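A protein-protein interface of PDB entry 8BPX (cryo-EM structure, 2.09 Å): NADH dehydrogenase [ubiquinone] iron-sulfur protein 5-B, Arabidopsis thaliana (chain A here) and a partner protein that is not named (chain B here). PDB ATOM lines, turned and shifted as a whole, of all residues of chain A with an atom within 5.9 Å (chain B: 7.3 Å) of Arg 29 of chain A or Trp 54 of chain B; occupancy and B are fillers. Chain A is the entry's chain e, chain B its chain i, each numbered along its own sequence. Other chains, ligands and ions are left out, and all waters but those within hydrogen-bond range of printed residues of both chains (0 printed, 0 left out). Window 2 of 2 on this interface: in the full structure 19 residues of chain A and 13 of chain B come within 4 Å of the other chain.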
ATOM      1  N   MET A  25     -24.737  29.007 -11.626  1.00  0.00           N
ATOM      2  CA  MET A  25     -24.832  29.113 -13.078  1.00  0.00           C
ATOM      3  C   MET A  25     -23.799  28.254 -13.798  1.00  0.00           C
ATOM      4  O   MET A  25     -24.001  27.919 -14.968  1.00  0.00           O
ATOM      5  CB  MET A  25     -24.697  30.577 -13.507  1.00  0.00           C
ATOM      6  CG  MET A  25     -25.958  31.396 -13.249  1.00  0.00           C
ATOM      7  SD  MET A  25     -27.028  31.667 -14.680  1.00  0.00           S
ATOM      8  CE  MET A  25     -25.867  32.312 -15.879  1.00  0.00           C
ATOM      9  N   SER A  26     -22.707  27.879 -13.128  1.00  0.00           N
ATOM     10  CA  SER A  26     -21.671  27.081 -13.771  1.00  0.00           C
ATOM     11  C   SER A  26     -22.104  25.656 -14.086  1.00  0.00           C
ATOM     12  O   SER A  26     -21.382  24.964 -14.810  1.00  0.00           O
ATOM     13  CB  SER A  26     -20.423  27.034 -12.892  1.00  0.00           C
ATOM     14  OG  SER A  26     -20.543  26.019 -11.911  1.00  0.00           O
ATOM     15  N   HIS A  27     -23.226  25.183 -13.547  1.00  0.00           N
ATOM     16  CA  HIS A  27     -23.684  23.837 -13.858  1.00  0.00           C
ATOM     17  C   HIS A  27     -25.171  23.732 -14.154  1.00  0.00           C
ATOM     18  O   HIS A  27     -25.611  22.667 -14.598  1.00  0.00           O
ATOM     19  CB  HIS A  27     -23.330  22.872 -12.716  1.00  0.00           C
ATOM     20  CG  HIS A  27     -23.761  23.349 -11.368  1.00  0.00           C
ATOM     21  ND1 HIS A  27     -25.087  23.448 -11.001  1.00  0.00           N
ATOM     22  CD2 HIS A  27     -23.042  23.748 -10.296  1.00  0.00           C
ATOM     23  CE1 HIS A  27     -25.163  23.891  -9.760  1.00  0.00           C
ATOM     24  NE2 HIS A  27     -23.937  24.083  -9.310  1.00  0.00           N
ATOM     25  N   CYS A  28     -25.955  24.778 -13.927  1.00  0.00           N
ATOM     26  CA  CYS A  28     -27.378  24.755 -14.232  1.00  0.00           C
ATOM     27  C   CYS A  28     -27.580  25.236 -15.662  1.00  0.00           C
ATOM     28  O   CYS A  28     -27.297  26.396 -15.977  1.00  0.00           O
ATOM     29  CB  CYS A  28     -28.159  25.626 -13.249  1.00  0.00           C
ATOM     30  SG  CYS A  28     -28.356  24.907 -11.607  1.00  0.00           S
ATOM     31  N   ARG A  29     -28.072  24.346 -16.524  1.00  0.00           N
ATOM     32  CA  ARG A  29     -28.219  24.666 -17.939  1.00  0.00           C
ATOM     33  C   ARG A  29     -29.303  25.700 -18.207  1.00  0.00           C
ATOM     34  O   ARG A  29     -29.345  26.249 -19.312  1.00  0.00           O
ATOM     35  CB  ARG A  29     -28.502  23.388 -18.733  1.00  0.00           C
ATOM     36  CG  ARG A  29     -27.275  22.509 -18.932  1.00  0.00           C
ATOM     37  CD  ARG A  29     -27.564  21.341 -19.862  1.00  0.00           C
ATOM     38  NE  ARG A  29     -28.633  20.490 -19.357  1.00  0.00           N
ATOM     39  CZ  ARG A  29     -28.470  19.539 -18.447  1.00  0.00           C
ATOM     40  NH1 ARG A  29     -27.283  19.283 -17.922  1.00  0.00           N
ATOM     41  NH2 ARG A  29     -29.523  18.828 -18.054  1.00  0.00           N
ATOM     42  N   GLU A  30     -30.174  25.974 -17.238  1.00  0.00           N
ATOM     43  CA  GLU A  30     -31.202  27.001 -17.366  1.00  0.00           C
ATOM     44  C   GLU A  30     -30.962  28.094 -16.333  1.00  0.00           C
ATOM     45  O   GLU A  30     -30.951  27.803 -15.125  1.00  0.00           O
ATOM     46  CB  GLU A  30     -32.599  26.403 -17.191  1.00  0.00           C
ATOM     47  CG  GLU A  30     -33.056  25.542 -18.350  1.00  0.00           C
ATOM     48  CD  GLU A  30     -33.518  24.169 -17.906  1.00  0.00           C
ATOM     49  OE1 GLU A  30     -33.299  23.818 -16.728  1.00  0.00           O
ATOM     50  OE2 GLU A  30     -34.100  23.440 -18.737  1.00  0.00           O
ATOM     51  N   PRO A  31     -30.768  29.350 -16.742  1.00  0.00           N
ATOM     52  CA  PRO A  31     -30.525  30.413 -15.753  1.00  0.00           C
ATOM     53  C   PRO A  31     -31.689  30.643 -14.805  1.00  0.00           C
ATOM     54  O   PRO A  31     -31.474  31.170 -13.708  1.00  0.00           O
ATOM     55  CB  PRO A  31     -30.257  31.646 -16.626  1.00  0.00           C
ATOM     56  CG  PRO A  31     -30.972  31.354 -17.903  1.00  0.00           C
ATOM     57  CD  PRO A  31     -30.824  29.876 -18.114  1.00  0.00           C
ATOM     58  N   ARG B  49     -26.427  31.066 -29.972  1.00  0.00           N
ATOM     59  CA  ARG B  49     -26.173  31.020 -28.539  1.00  0.00           C
ATOM     60  C   ARG B  49     -26.458  29.606 -28.055  1.00  0.00           C
ATOM     61  O   ARG B  49     -27.630  29.230 -27.894  1.00  0.00           O
ATOM     62  CB  ARG B  49     -27.058  32.039 -27.814  1.00  0.00           C
ATOM     63  CG  ARG B  49     -26.712  32.304 -26.361  1.00  0.00           C
ATOM     64  CD  ARG B  49     -27.473  31.364 -25.436  1.00  0.00           C
ATOM     65  NE  ARG B  49     -28.916  31.540 -25.545  1.00  0.00           N
ATOM     66  CZ  ARG B  49     -29.811  30.800 -24.903  1.00  0.00           C
ATOM     67  NH1 ARG B  49     -29.443  29.824 -24.088  1.00  0.00           N
ATOM     68  NH2 ARG B  49     -31.105  31.048 -25.082  1.00  0.00           N
ATOM     69  N   PRO B  50     -25.396  28.783 -27.846  1.00  0.00           N
ATOM     70  CA  PRO B  50     -25.636  27.406 -27.457  1.00  0.00           C
ATOM     71  C   PRO B  50     -26.359  27.291 -26.105  1.00  0.00           C
ATOM     72  O   PRO B  50     -26.426  28.263 -25.397  1.00  0.00           O
ATOM     73  CB  PRO B  50     -24.200  26.834 -27.495  1.00  0.00           C
ATOM     74  CG  PRO B  50     -23.303  27.968 -27.185  1.00  0.00           C
ATOM     75  CD  PRO B  50     -23.951  29.080 -27.954  1.00  0.00           C
ATOM     76  N   TYR B  51     -26.900  26.137 -25.796  1.00  0.00           N
ATOM     77  CA  TYR B  51     -27.549  25.867 -24.521  1.00  0.00           C
ATOM     78  C   TYR B  51     -26.531  25.900 -23.390  1.00  0.00           C
ATOM     79  O   TYR B  51     -25.613  25.075 -23.345  1.00  0.00           O
ATOM     80  CB  TYR B  51     -28.238  24.505 -24.581  1.00  0.00           C
ATOM     81  CG  TYR B  51     -29.298  24.270 -23.530  1.00  0.00           C
ATOM     82  CD1 TYR B  51     -30.236  25.245 -23.224  1.00  0.00           C
ATOM     83  CD2 TYR B  51     -29.364  23.063 -22.848  1.00  0.00           C
ATOM     84  CE1 TYR B  51     -31.208  25.024 -22.268  1.00  0.00           C
ATOM     85  CE2 TYR B  51     -30.330  22.833 -21.895  1.00  0.00           C
ATOM     86  CZ  TYR B  51     -31.251  23.814 -21.608  1.00  0.00           C
ATOM     87  OH  TYR B  51     -32.212  23.581 -20.656  1.00  0.00           O
ATOM     88  N   GLY B  52     -26.698  26.852 -22.474  1.00  0.00           N
ATOM     89  CA  GLY B  52     -25.834  26.946 -21.314  1.00  0.00           C
ATOM     90  C   GLY B  52     -24.375  27.173 -21.651  1.00  0.00           C
ATOM     91  O   GLY B  52     -23.506  26.461 -21.145  1.00  0.00           O
ATOM     92  N   PHE B  53     -24.090  28.148 -22.518  1.00  0.00           N
ATOM     93  CA  PHE B  53     -22.705  28.387 -22.911  1.00  0.00           C
ATOM     94  C   PHE B  53     -21.853  28.789 -21.712  1.00  0.00           C
ATOM     95  O   PHE B  53     -20.690  28.389 -21.608  1.00  0.00           O
ATOM     96  CB  PHE B  53     -22.636  29.454 -24.003  1.00  0.00           C
ATOM     97  CG  PHE B  53     -23.171  30.793 -23.585  1.00  0.00           C
ATOM     98  CD1 PHE B  53     -24.523  31.075 -23.675  1.00  0.00           C
ATOM     99  CD2 PHE B  53     -22.320  31.775 -23.108  1.00  0.00           C
ATOM    100  CE1 PHE B  53     -25.011  32.309 -23.291  1.00  0.00           C
ATOM    101  CE2 PHE B  53     -22.807  33.007 -22.724  1.00  0.00           C
ATOM    102  CZ  PHE B  53     -24.149  33.275 -22.816  1.00  0.00           C
ATOM    103  N   TRP B  54     -22.427  29.553 -20.780  1.00  0.00           N
ATOM    104  CA  TRP B  54     -21.704  29.978 -19.587  1.00  0.00           C
ATOM    105  C   TRP B  54     -21.305  28.809 -18.693  1.00  0.00           C
ATOM    106  O   TRP B  54     -20.483  28.997 -17.790  1.00  0.00           O
ATOM    107  CB  TRP B  54     -22.548  30.982 -18.801  1.00  0.00           C
ATOM    108  CG  TRP B  54     -23.841  30.402 -18.345  1.00  0.00           C
ATOM    109  CD1 TRP B  54     -24.068  29.731 -17.190  1.00  0.00           C
ATOM    110  CD2 TRP B  54     -25.084  30.413 -19.056  1.00  0.00           C
ATOM    111  NE1 TRP B  54     -25.379  29.326 -17.125  1.00  0.00           N
ATOM    112  CE2 TRP B  54     -26.025  29.733 -18.261  1.00  0.00           C
ATOM    113  CE3 TRP B  54     -25.492  30.934 -20.285  1.00  0.00           C
ATOM    114  CZ2 TRP B  54     -27.351  29.567 -18.652  1.00  0.00           C
ATOM    115  CZ3 TRP B  54     -26.807  30.766 -20.674  1.00  0.00           C
ATOM    116  CH2 TRP B  54     -27.721  30.088 -19.860  1.00  0.00           C
ATOM    117  N   THR B  55     -21.872  27.622 -18.913  1.00  0.00           N
ATOM    118  CA  THR B  55     -21.417  26.409 -18.242  1.00  0.00           C
ATOM    119  C   THR B  55     -20.067  25.922 -18.757  1.00  0.00           C
ATOM    120  O   THR B  55     -19.337  25.259 -18.012  1.00  0.00           O
ATOM    121  CB  THR B  55     -22.474  25.309 -18.409  1.00  0.00           C
ATOM    122  OG1 THR B  55     -23.735  25.782 -17.922  1.00  0.00           O
ATOM    123  CG2 THR B  55     -22.091  24.039 -17.664  1.00  0.00           C
ATOM    124  N   PHE B  56     -19.713  26.234 -20.018  1.00  0.00           N
ATOM    125  CA  PHE B  56     -18.482  25.752 -20.671  1.00  0.00           C
ATOM    126  C   PHE B  56     -17.241  26.235 -19.885  1.00  0.00           C
ATOM    127  O   PHE B  56     -17.205  27.419 -19.505  1.00  0.00           O
ATOM    128  CB  PHE B  56     -18.504  26.126 -22.146  1.00  0.00           C
ATOM    129  CG  PHE B  56     -19.699  25.736 -22.977  1.00  0.00           C
ATOM    130  CD1 PHE B  56     -20.545  24.708 -22.603  1.00  0.00           C
ATOM    131  CD2 PHE B  56     -19.976  26.417 -24.150  1.00  0.00           C
ATOM    132  CE1 PHE B  56     -21.645  24.378 -23.375  1.00  0.00           C
ATOM    133  CE2 PHE B  56     -21.086  26.096 -24.917  1.00  0.00           C
ATOM    134  CZ  PHE B  56     -21.912  25.072 -24.528  1.00  0.00           C
ATOM    135  N   GLU B  57     -16.271  25.360 -19.653  1.00  0.00           N
ATOM    136  CA  GLU B  57     -15.157  25.598 -18.739  1.00  0.00           C
ATOM    137  C   GLU B  57     -14.424  26.896 -19.046  1.00  0.00           C
ATOM    138  O   GLU B  57     -13.939  27.563 -18.125  1.00  0.00           O
ATOM    139  CB  GLU B  57     -14.184  24.419 -18.784  1.00  0.00           C
ATOM    140  CG  GLU B  57     -14.633  23.216 -17.972  1.00  0.00           C
ATOM    141  CD  GLU B  57     -15.760  22.447 -18.638  1.00  0.00           C
ATOM    142  OE1 GLU B  57     -15.970  22.631 -19.856  1.00  0.00           O
ATOM    143  OE2 GLU B  57     -16.436  21.659 -17.943  1.00  0.00           O
ATOM    144  N   ARG B  58     -14.328  27.272 -20.325  1.00  0.00           N
ATOM    145  CA  ARG B  58     -13.674  28.526 -20.682  1.00  0.00           C
ATOM    146  C   ARG B  58     -14.324  29.717 -19.985  1.00  0.00           C
ATOM    147  O   ARG B  58     -13.651  30.713 -19.699  1.00  0.00           O
ATOM    148  CB  ARG B  58     -13.698  28.715 -22.200  1.00  0.00           C
ATOM    149  CG  ARG B  58     -13.297  30.104 -22.679  1.00  0.00           C
ATOM    150  CD  ARG B  58     -11.815  30.363 -22.455  1.00  0.00           C
ATOM    151  NE  ARG B  58     -11.535  30.954 -21.152  1.00  0.00           N
ATOM    152  CZ  ARG B  58     -10.318  31.121 -20.652  1.00  0.00           C
ATOM    153  NH1 ARG B  58      -9.239  30.762 -21.326  1.00  0.00           N
ATOM    154  NH2 ARG B  58     -10.181  31.666 -19.447  1.00  0.00           N
ATOM    155  N   HIS B  59     -15.600  29.588 -19.656  1.00  0.00           N
ATOM    156  CA  HIS B  59     -16.330  30.728 -19.081  1.00  0.00           C
ATOM    157  C   HIS B  59     -16.334  30.717 -17.536  1.00  0.00           C
ATOM    158  O   HIS B  59     -16.862  31.627 -16.943  1.00  0.00           O
ATOM    159  CB  HIS B  59     -17.693  30.699 -19.701  1.00  0.00           C
ATOM    160  CG  HIS B  59     -17.755  30.612 -21.194  1.00  0.00           C
ATOM    161  ND1 HIS B  59     -18.950  30.613 -21.867  1.00  0.00           N
ATOM    162  CD2 HIS B  59     -16.801  30.502 -22.142  1.00  0.00           C
ATOM    163  CE1 HIS B  59     -18.734  30.507 -23.159  1.00  0.00           C
ATOM    164  NE2 HIS B  59     -17.424  30.431 -23.354  1.00  0.00           N
ATOM    165  N   ASN B  60     -15.808  29.677 -16.937  1.00  0.00           N
ATOM    166  CA  ASN B  60     -15.778  29.558 -15.484  1.00  0.00           C
ATOM    167  C   ASN B  60     -14.384  29.848 -14.936  1.00  0.00           C
ATOM    168  O   ASN B  60     -13.938  29.232 -13.967  1.00  0.00           O
ATOM    169  CB  ASN B  60     -16.249  28.175 -15.043  1.00  0.00           C
ATOM    170  CG  ASN B  60     -17.734  27.962 -15.273  1.00  0.00           C
ATOM    171  OD1 ASN B  60     -18.509  28.917 -15.345  1.00  0.00           O
ATOM    172  ND2 ASN B  60     -18.139  26.701 -15.391  1.00  0.00           N
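The indole nitrogen (NE1) of Trp 54 of chain B lies close to the backbone carbonyl oxygen (O) of Met 25 of chain A, 2.9 Å away.
The side-chain carboxylate (OE2) of Glu 30 of chain A lies within hydrogen-bond range of the side-chain hydroxyl (OH) of Tyr 51 of chain B (2.7 Å).
The backbone carbonyl oxygen (O) of Gly 52 of chain B sits close to the side-chain hydroxyl (OG1) of Thr 55 of chain B.
O of Trp 54 of chain B sits close to OD1 of Asn 60 of chain B (3.1 Å).
SG of Cys 28 of chain A is in hydrogen-bond range of ND1 of His 27 of chain A (3.6 Å).
O of Thr 55 of chain B sits at hydrogen-bond distance from ND2 of Asn 60 of chain B, at 3.2 Å.
Met 25 of chain A touches Thr 55 of chain B (O to OG1, 3.7 Å).
Thr 55 of chain B touches Ser 26 of chain A (CG2 to O, 3.1 Å).
Ser 26 of chain A touches Asn 60 of chain B (CB to ND2, 3.4 Å).
NE1 of Trp 54 of chain B touches O of Cys 28 of chain A (3.7 Å).
CE2 of Tyr 51 of chain B touches CB of Arg 29 of chain A, 3.7 Å away.
CZ2 of Trp 54 of chain B touches O of Arg 29 of chain A, at 3.9 Å.
CD of Pro 31 of chain A touches CZ2 of Trp 54 of chain B, at 3.5 Å.
Printed residues of chain B within 4 Å of Ser 26 of chain A: Thr 55 (3.1 Å) and Asn 60 (3.4 Å).
Of the printed residues of chain B, Cys 28 of chain A touches Trp 54 (3.7 Å).
Printed residues of chain B within 4 Å of Arg 29 of chain A: Tyr 51 (3.7 Å) and Trp 54 (3.9 Å).
Printed residues of chain B within 4 Å of Pro 31 of chain A: Trp 54 (3.5 Å).
Phe 53 of chain B touches none of the printed residues of chain A.
Printed residues of chain A within 4 Å of Thr 55 of chain B: Met 25 and Ser 26.
Of the printed residues of chain A, Asn 60 of chain B touches Ser 26.
The nearest residue of chain B that does not touch Arg 29 of chain A is Gly 52 of chain B (4.1 Å).
The nearest residue of chain A that does not touch Trp 54 of chain B is Glu 30 of chain A (4.5 Å).
The nearest printed residue of chain A that does not touch Asn 60 of chain B is Met 25 of chain A (5.6 Å).
Hydrophobic or aromatic side chains of chain A that line the printed part of chain B: Met 25 and Pro 31.
Hydrophobic or aromatic side chains of chain B within 4 Å of the printed part of chain A: Tyr 51 and Trp 54.
Among the printed residues, 9 pairs touch across the chains.
Among the printed residues, no Asp or Glu carboxylate lies within 4 Å of a Lys or Arg side-chain nitrogen of the other chain.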
